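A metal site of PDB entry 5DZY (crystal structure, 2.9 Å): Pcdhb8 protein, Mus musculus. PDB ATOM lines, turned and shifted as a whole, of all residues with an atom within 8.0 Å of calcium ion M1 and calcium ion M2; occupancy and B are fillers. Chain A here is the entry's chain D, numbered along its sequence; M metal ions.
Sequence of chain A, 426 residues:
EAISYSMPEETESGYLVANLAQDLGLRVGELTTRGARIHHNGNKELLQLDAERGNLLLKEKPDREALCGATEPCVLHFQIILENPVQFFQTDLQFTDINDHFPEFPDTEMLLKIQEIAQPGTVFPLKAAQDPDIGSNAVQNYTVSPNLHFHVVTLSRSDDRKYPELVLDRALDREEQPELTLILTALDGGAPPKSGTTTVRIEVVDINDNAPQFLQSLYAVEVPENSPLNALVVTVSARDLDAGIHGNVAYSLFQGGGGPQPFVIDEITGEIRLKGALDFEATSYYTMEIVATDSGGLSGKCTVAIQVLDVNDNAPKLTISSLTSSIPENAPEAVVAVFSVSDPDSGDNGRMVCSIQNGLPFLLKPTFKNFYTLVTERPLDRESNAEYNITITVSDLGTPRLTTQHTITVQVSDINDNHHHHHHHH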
ATOM      1  N   GLU A   9     -16.082   2.376 -16.065  1.00  0.00           N
ATOM      2  CA  GLU A   9     -17.152   1.542 -15.551  1.00  0.00           C
ATOM      3  C   GLU A   9     -17.025   0.108 -16.073  1.00  0.00           C
ATOM      4  O   GLU A   9     -16.452  -0.120 -17.135  1.00  0.00           O
ATOM      5  CB  GLU A   9     -18.521   2.136 -15.934  1.00  0.00           C
ATOM      6  CG  GLU A   9     -19.715   1.442 -15.304  1.00  0.00           C
ATOM      7  CD  GLU A   9     -21.027   1.871 -15.928  1.00  0.00           C
ATOM      8  OE1 GLU A   9     -21.008   2.783 -16.778  1.00  0.00           O
ATOM      9  OE2 GLU A   9     -22.080   1.284 -15.579  1.00  0.00           O
ATOM     10  N   GLU A  10     -17.564  -0.845 -15.304  1.00  0.00           N
ATOM     11  CA  GLU A  10     -17.593  -2.248 -15.690  1.00  0.00           C
ATOM     12  C   GLU A  10     -16.202  -2.819 -15.924  1.00  0.00           C
ATOM     13  O   GLU A  10     -15.986  -3.597 -16.865  1.00  0.00           O
ATOM     14  CB  GLU A  10     -18.459  -2.448 -16.941  1.00  0.00           C
ATOM     15  CG  GLU A  10     -19.923  -2.105 -16.759  1.00  0.00           C
ATOM     16  CD  GLU A  10     -20.689  -3.163 -15.980  1.00  0.00           C
ATOM     17  OE1 GLU A  10     -20.096  -4.202 -15.642  1.00  0.00           O
ATOM     18  OE2 GLU A  10     -21.885  -2.942 -15.703  1.00  0.00           O
ATOM     19  N   PRO A  62     -18.036  -3.256 -10.927  1.00  0.00           N
ATOM     20  CA  PRO A  62     -18.836  -2.068 -10.593  1.00  0.00           C
ATOM     21  C   PRO A  62     -19.743  -1.608 -11.733  1.00  0.00           C
ATOM     22  O   PRO A  62     -19.296  -1.456 -12.876  1.00  0.00           O
ATOM     23  CB  PRO A  62     -17.778  -1.018 -10.280  1.00  0.00           C
ATOM     24  CG  PRO A  62     -16.630  -1.393 -11.139  1.00  0.00           C
ATOM     25  CD  PRO A  62     -16.636  -2.895 -11.241  1.00  0.00           C
ATOM     26  N   ASP A  63     -21.015  -1.384 -11.414  1.00  0.00           N
ATOM     27  CA  ASP A  63     -21.964  -0.823 -12.376  1.00  0.00           C
ATOM     28  C   ASP A  63     -22.465   0.530 -11.869  1.00  0.00           C
ATOM     29  O   ASP A  63     -23.029   0.618 -10.783  1.00  0.00           O
ATOM     30  CB  ASP A  63     -23.137  -1.773 -12.619  1.00  0.00           C
ATOM     31  CG  ASP A  63     -24.173  -1.181 -13.545  1.00  0.00           C
ATOM     32  OD1 ASP A  63     -24.084  -1.385 -14.767  1.00  0.00           O
ATOM     33  OD2 ASP A  63     -25.095  -0.502 -13.042  1.00  0.00           O
ATOM     34  N   ARG A  64     -22.270   1.572 -12.673  1.00  0.00           N
ATOM     35  CA  ARG A  64     -22.642   2.926 -12.286  1.00  0.00           C
ATOM     36  C   ARG A  64     -24.149   3.059 -12.085  1.00  0.00           C
ATOM     37  O   ARG A  64     -24.601   3.597 -11.071  1.00  0.00           O
ATOM     38  CB  ARG A  64     -22.151   3.919 -13.352  1.00  0.00           C
ATOM     39  CG  ARG A  64     -21.856   5.327 -12.842  1.00  0.00           C
ATOM     40  CD  ARG A  64     -23.118   6.128 -12.559  1.00  0.00           C
ATOM     41  NE  ARG A  64     -24.115   5.956 -13.609  1.00  0.00           N
ATOM     42  CZ  ARG A  64     -24.178   6.716 -14.707  1.00  0.00           C
ATOM     43  NH1 ARG A  64     -23.301   7.687 -14.896  1.00  0.00           N
ATOM     44  NH2 ARG A  64     -25.116   6.487 -15.610  1.00  0.00           N
ATOM     45  N   GLU A  65     -24.915   2.566 -13.055  1.00  0.00           N
ATOM     46  CA  GLU A  65     -26.361   2.779 -13.069  1.00  0.00           C
ATOM     47  C   GLU A  65     -27.079   2.004 -11.956  1.00  0.00           C
ATOM     48  O   GLU A  65     -28.178   2.403 -11.534  1.00  0.00           O
ATOM     49  CB  GLU A  65     -26.932   2.369 -14.427  1.00  0.00           C
ATOM     50  CG  GLU A  65     -26.531   3.284 -15.585  1.00  0.00           C
ATOM     51  CD  GLU A  65     -25.098   3.079 -16.022  1.00  0.00           C
ATOM     52  OE1 GLU A  65     -24.602   1.931 -15.927  1.00  0.00           O
ATOM     53  OE2 GLU A  65     -24.459   4.054 -16.461  1.00  0.00           O
ATOM     54  N   ALA A  66     -26.472   0.926 -11.490  1.00  0.00           N
ATOM     55  CA  ALA A  66     -27.087   0.115 -10.436  1.00  0.00           C
ATOM     56  C   ALA A  66     -26.587   0.521  -9.059  1.00  0.00           C
ATOM     57  O   ALA A  66     -27.048  -0.007  -8.040  1.00  0.00           O
ATOM     58  CB  ALA A  66     -26.810  -1.359 -10.684  1.00  0.00           C
ATOM     59  N   THR A  96     -15.748   6.526 -14.109  1.00  0.00           N
ATOM     60  CA  THR A  96     -16.002   7.232 -15.361  1.00  0.00           C
ATOM     61  C   THR A  96     -17.083   6.511 -16.159  1.00  0.00           C
ATOM     62  O   THR A  96     -16.990   5.309 -16.404  1.00  0.00           O
ATOM     63  CB  THR A  96     -14.723   7.343 -16.216  1.00  0.00           C
ATOM     64  OG1 THR A  96     -13.738   8.109 -15.510  1.00  0.00           O
ATOM     65  CG2 THR A  96     -15.024   8.015 -17.541  1.00  0.00           C
ATOM     66  N   ASP A  97     -18.104   7.265 -16.557  1.00  0.00           N
ATOM     67  CA  ASP A  97     -19.214   6.697 -17.315  1.00  0.00           C
ATOM     68  C   ASP A  97     -18.744   6.161 -18.657  1.00  0.00           C
ATOM     69  O   ASP A  97     -17.938   6.787 -19.344  1.00  0.00           O
ATOM     70  CB  ASP A  97     -20.307   7.758 -17.519  1.00  0.00           C
ATOM     71  CG  ASP A  97     -21.639   7.165 -17.960  1.00  0.00           C
ATOM     72  OD1 ASP A  97     -21.663   6.003 -18.419  1.00  0.00           O
ATOM     73  OD2 ASP A  97     -22.664   7.854 -17.832  1.00  0.00           O
ATOM     74  N   ILE A  98     -19.254   4.994 -19.028  1.00  0.00           N
ATOM     75  CA  ILE A  98     -18.947   4.388 -20.321  1.00  0.00           C
ATOM     76  C   ILE A  98     -20.248   4.130 -21.082  1.00  0.00           C
ATOM     77  O   ILE A  98     -21.285   3.824 -20.476  1.00  0.00           O
ATOM     78  CB  ILE A  98     -18.133   3.083 -20.175  1.00  0.00           C
ATOM     79  CG1 ILE A  98     -17.582   2.623 -21.529  1.00  0.00           C
ATOM     80  CG2 ILE A  98     -18.971   1.987 -19.521  1.00  0.00           C
ATOM     81  CD1 ILE A  98     -16.647   3.616 -22.183  1.00  0.00           C
ATOM     82  N   ASN A  99     -20.206   4.270 -22.397  1.00  0.00           N
ATOM     83  CA  ASN A  99     -21.380   4.013 -23.226  1.00  0.00           C
ATOM     84  C   ASN A  99     -21.647   2.517 -23.325  1.00  0.00           C
ATOM     85  O   ASN A  99     -21.272   1.870 -24.297  1.00  0.00           O
ATOM     86  CB  ASN A  99     -21.191   4.613 -24.617  1.00  0.00           C
ATOM     87  CG  ASN A  99     -22.455   4.548 -25.462  1.00  0.00           C
ATOM     88  OD1 ASN A  99     -23.553   4.409 -24.933  1.00  0.00           O
ATOM     89  ND2 ASN A  99     -22.289   4.672 -26.770  1.00  0.00           N
ATOM     90  N   ASP A 100     -22.313   1.974 -22.312  1.00  0.00           N
ATOM     91  CA  ASP A 100     -22.563   0.534 -22.242  1.00  0.00           C
ATOM     92  C   ASP A 100     -24.058   0.209 -22.268  1.00  0.00           C
ATOM     93  O   ASP A 100     -24.485  -0.837 -21.788  1.00  0.00           O
ATOM     94  CB  ASP A 100     -21.934  -0.061 -20.979  1.00  0.00           C
ATOM     95  CG  ASP A 100     -22.528   0.508 -19.702  1.00  0.00           C
ATOM     96  OD1 ASP A 100     -23.019   1.653 -19.739  1.00  0.00           O
ATOM     97  OD2 ASP A 100     -22.505  -0.197 -18.675  1.00  0.00           O
ATOM     98  N   HIS A 101     -24.851   1.109 -22.838  1.00  0.00           N
ATOM     99  CA  HIS A 101     -26.291   0.909 -22.935  1.00  0.00           C
ATOM    100  C   HIS A 101     -26.820   1.214 -24.338  1.00  0.00           C
ATOM    101  O   HIS A 101     -26.415   2.189 -24.969  1.00  0.00           O
ATOM    102  CB  HIS A 101     -27.024   1.776 -21.906  1.00  0.00           C
ATOM    103  CG  HIS A 101     -27.384   1.046 -20.646  1.00  0.00           C
ATOM    104  ND1 HIS A 101     -26.431   0.643 -19.729  1.00  0.00           N
ATOM    105  CD2 HIS A 101     -28.570   0.639 -20.153  1.00  0.00           C
ATOM    106  CE1 HIS A 101     -27.021   0.035 -18.724  1.00  0.00           C
ATOM    107  NE2 HIS A 101     -28.327   0.014 -18.963  1.00  0.00           N
ATOM    108  N   ASP A 131     -32.397   6.015 -21.758  1.00  0.00           N
ATOM    109  CA  ASP A 131     -30.957   5.764 -21.658  1.00  0.00           C
ATOM    110  C   ASP A 131     -30.454   6.146 -20.263  1.00  0.00           C
ATOM    111  O   ASP A 131     -30.356   7.337 -19.944  1.00  0.00           O
ATOM    112  CB  ASP A 131     -30.198   6.538 -22.739  1.00  0.00           C
ATOM    113  CG  ASP A 131     -28.812   5.970 -22.996  1.00  0.00           C
ATOM    114  OD1 ASP A 131     -28.246   5.317 -22.090  1.00  0.00           O
ATOM    115  OD2 ASP A 131     -28.295   6.163 -24.123  1.00  0.00           O
ATOM    116  N   PRO A 132     -30.140   5.143 -19.431  1.00  0.00           N
ATOM    117  CA  PRO A 132     -29.681   5.331 -18.058  1.00  0.00           C
ATOM    118  C   PRO A 132     -28.332   6.054 -17.951  1.00  0.00           C
ATOM    119  O   PRO A 132     -27.921   6.394 -16.839  1.00  0.00           O
ATOM    120  CB  PRO A 132     -29.554   3.892 -17.527  1.00  0.00           C
ATOM    121  CG  PRO A 132     -30.442   3.080 -18.419  1.00  0.00           C
ATOM    122  CD  PRO A 132     -30.320   3.718 -19.762  1.00  0.00           C
ATOM    123  N   ASP A 133     -27.668   6.277 -19.075  1.00  0.00           N
ATOM    124  CA  ASP A 133     -26.377   6.957 -19.082  1.00  0.00           C
ATOM    125  C   ASP A 133     -26.537   8.455 -18.815  1.00  0.00           C
ATOM    126  O   ASP A 133     -27.647   8.975 -18.827  1.00  0.00           O
ATOM    127  CB  ASP A 133     -25.661   6.736 -20.408  1.00  0.00           C
ATOM    128  CG  ASP A 133     -25.473   5.260 -20.731  1.00  0.00           C
ATOM    129  OD1 ASP A 133     -25.413   4.445 -19.784  1.00  0.00           O
ATOM    130  OD2 ASP A 133     -25.362   4.919 -21.929  1.00  0.00           O
ATOM    131  N   ILE A 134     -25.417   9.130 -18.571  1.00  0.00           N
ATOM    132  CA  ILE A 134     -25.423  10.556 -18.262  1.00  0.00           C
ATOM    133  C   ILE A 134     -24.465  11.328 -19.159  1.00  0.00           C
ATOM    134  O   ILE A 134     -23.334  10.889 -19.395  1.00  0.00           O
ATOM    135  CB  ILE A 134     -25.054  10.812 -16.783  1.00  0.00           C
ATOM    136  CG1 ILE A 134     -25.982  10.020 -15.850  1.00  0.00           C
ATOM    137  CG2 ILE A 134     -25.129  12.300 -16.460  1.00  0.00           C
ATOM    138  CD1 ILE A 134     -25.684  10.234 -14.387  1.00  0.00           C
ATOM    139  N   ASN A 137     -22.921  10.215 -23.019  1.00  0.00           N
ATOM    140  CA  ASN A 137     -23.074   8.767 -23.117  1.00  0.00           C
ATOM    141  C   ASN A 137     -24.537   8.351 -23.304  1.00  0.00           C
ATOM    142  O   ASN A 137     -24.832   7.168 -23.483  1.00  0.00           O
ATOM    143  CB  ASN A 137     -22.492   8.077 -21.875  1.00  0.00           C
ATOM    144  CG  ASN A 137     -21.010   8.351 -21.711  1.00  0.00           C
ATOM    145  OD1 ASN A 137     -20.579   8.843 -20.667  1.00  0.00           O
ATOM    146  ND2 ASN A 137     -20.228   8.023 -22.729  1.00  0.00           N
ATOM    147  N   ALA A 138     -25.435   9.326 -23.260  1.00  0.00           N
ATOM    148  CA  ALA A 138     -26.854   9.067 -23.426  1.00  0.00           C
ATOM    149  C   ALA A 138     -27.297   9.350 -24.859  1.00  0.00           C
ATOM    150  O   ALA A 138     -26.472   9.635 -25.726  1.00  0.00           O
ATOM    151  CB  ALA A 138     -27.671   9.899 -22.442  1.00  0.00           C
HETATM  152 CA    CA M   1     -24.406  -0.513 -17.127  1.00  0.00          CA
HETATM  153 CA    CA M   2     -22.919   3.751 -18.403  1.00  0.00          CA
HETATM  154 CA    CA M   3     -26.241   4.583 -24.443  1.00  0.00          CA
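The side-chain carboxylate (OE2) of Glu 65 sits close to the guanidinium group (NH2) of Arg 64, at 2.7 Å. OD2 of Asp 63 is in hydrogen-bond range of N of Ala 66 (2.5 Å). The guanidinium group of Arg 64 is in salt-bridge range of the side-chain carboxylate of Asp 97 (3.0 Å). The side-chain carboxylate (OD2) of Asp 97 lies within hydrogen-bond range of the backbone NH (N) of Ile 134, 3.1 Å away. N of Arg 64 sits at hydrogen-bond distance from OE2 of Glu 9, 2.9 Å away. The backbone NH (N) of Glu 9 lies within hydrogen-bond range of the backbone carbonyl oxygen (O) of Thr 96, at 3.1 Å. O of Pro 62 sits at hydrogen-bond distance from N of Glu 10 (3.0 Å).
Calcium ion M1 is bound by OD2 of Asp 100, OD1 of Asp 63 and OE1 of Glu 65. Calcium ion M1 has three donor atoms within binding distance.
Within 4 Å of calcium ion M2: Glu 9, Glu 65, Asp 97, Ile 98, Asp 100 and Asp 133. Along chain A the residues within 4 Å of calcium ion M2 span positions 9 to 133.
Calcium ion M2 is bound by the side-chain carboxylate (OD1) of Asp 100 (2.5 Å), the side-chain carboxylate (OE2) of Glu 65 (2.5 Å), the side-chain carboxylate (OD1) of Asp 97 (2.6 Å), the backbone carbonyl oxygen (O) of Ile 98 (2.6 Å) and the side-chain carboxylate (OE1) of Glu 9 (2.7 Å). Slightly farther from calcium ion M2 lies the side-chain carboxylate (OD1) of Asp 133 (2.9 Å).
OE2 of Glu 10 touches calcium ion M1, 3.8 Å away. His 101 touches calcium ion M1. Six residues have an atom within 4 Å of calcium ion M1: Glu 9, Glu 10, Asp 63, Glu 65, Asp 100 and His 101. The nearest printed residue that does not touch calcium ion M1 is Arg 64 (5.4 Å).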
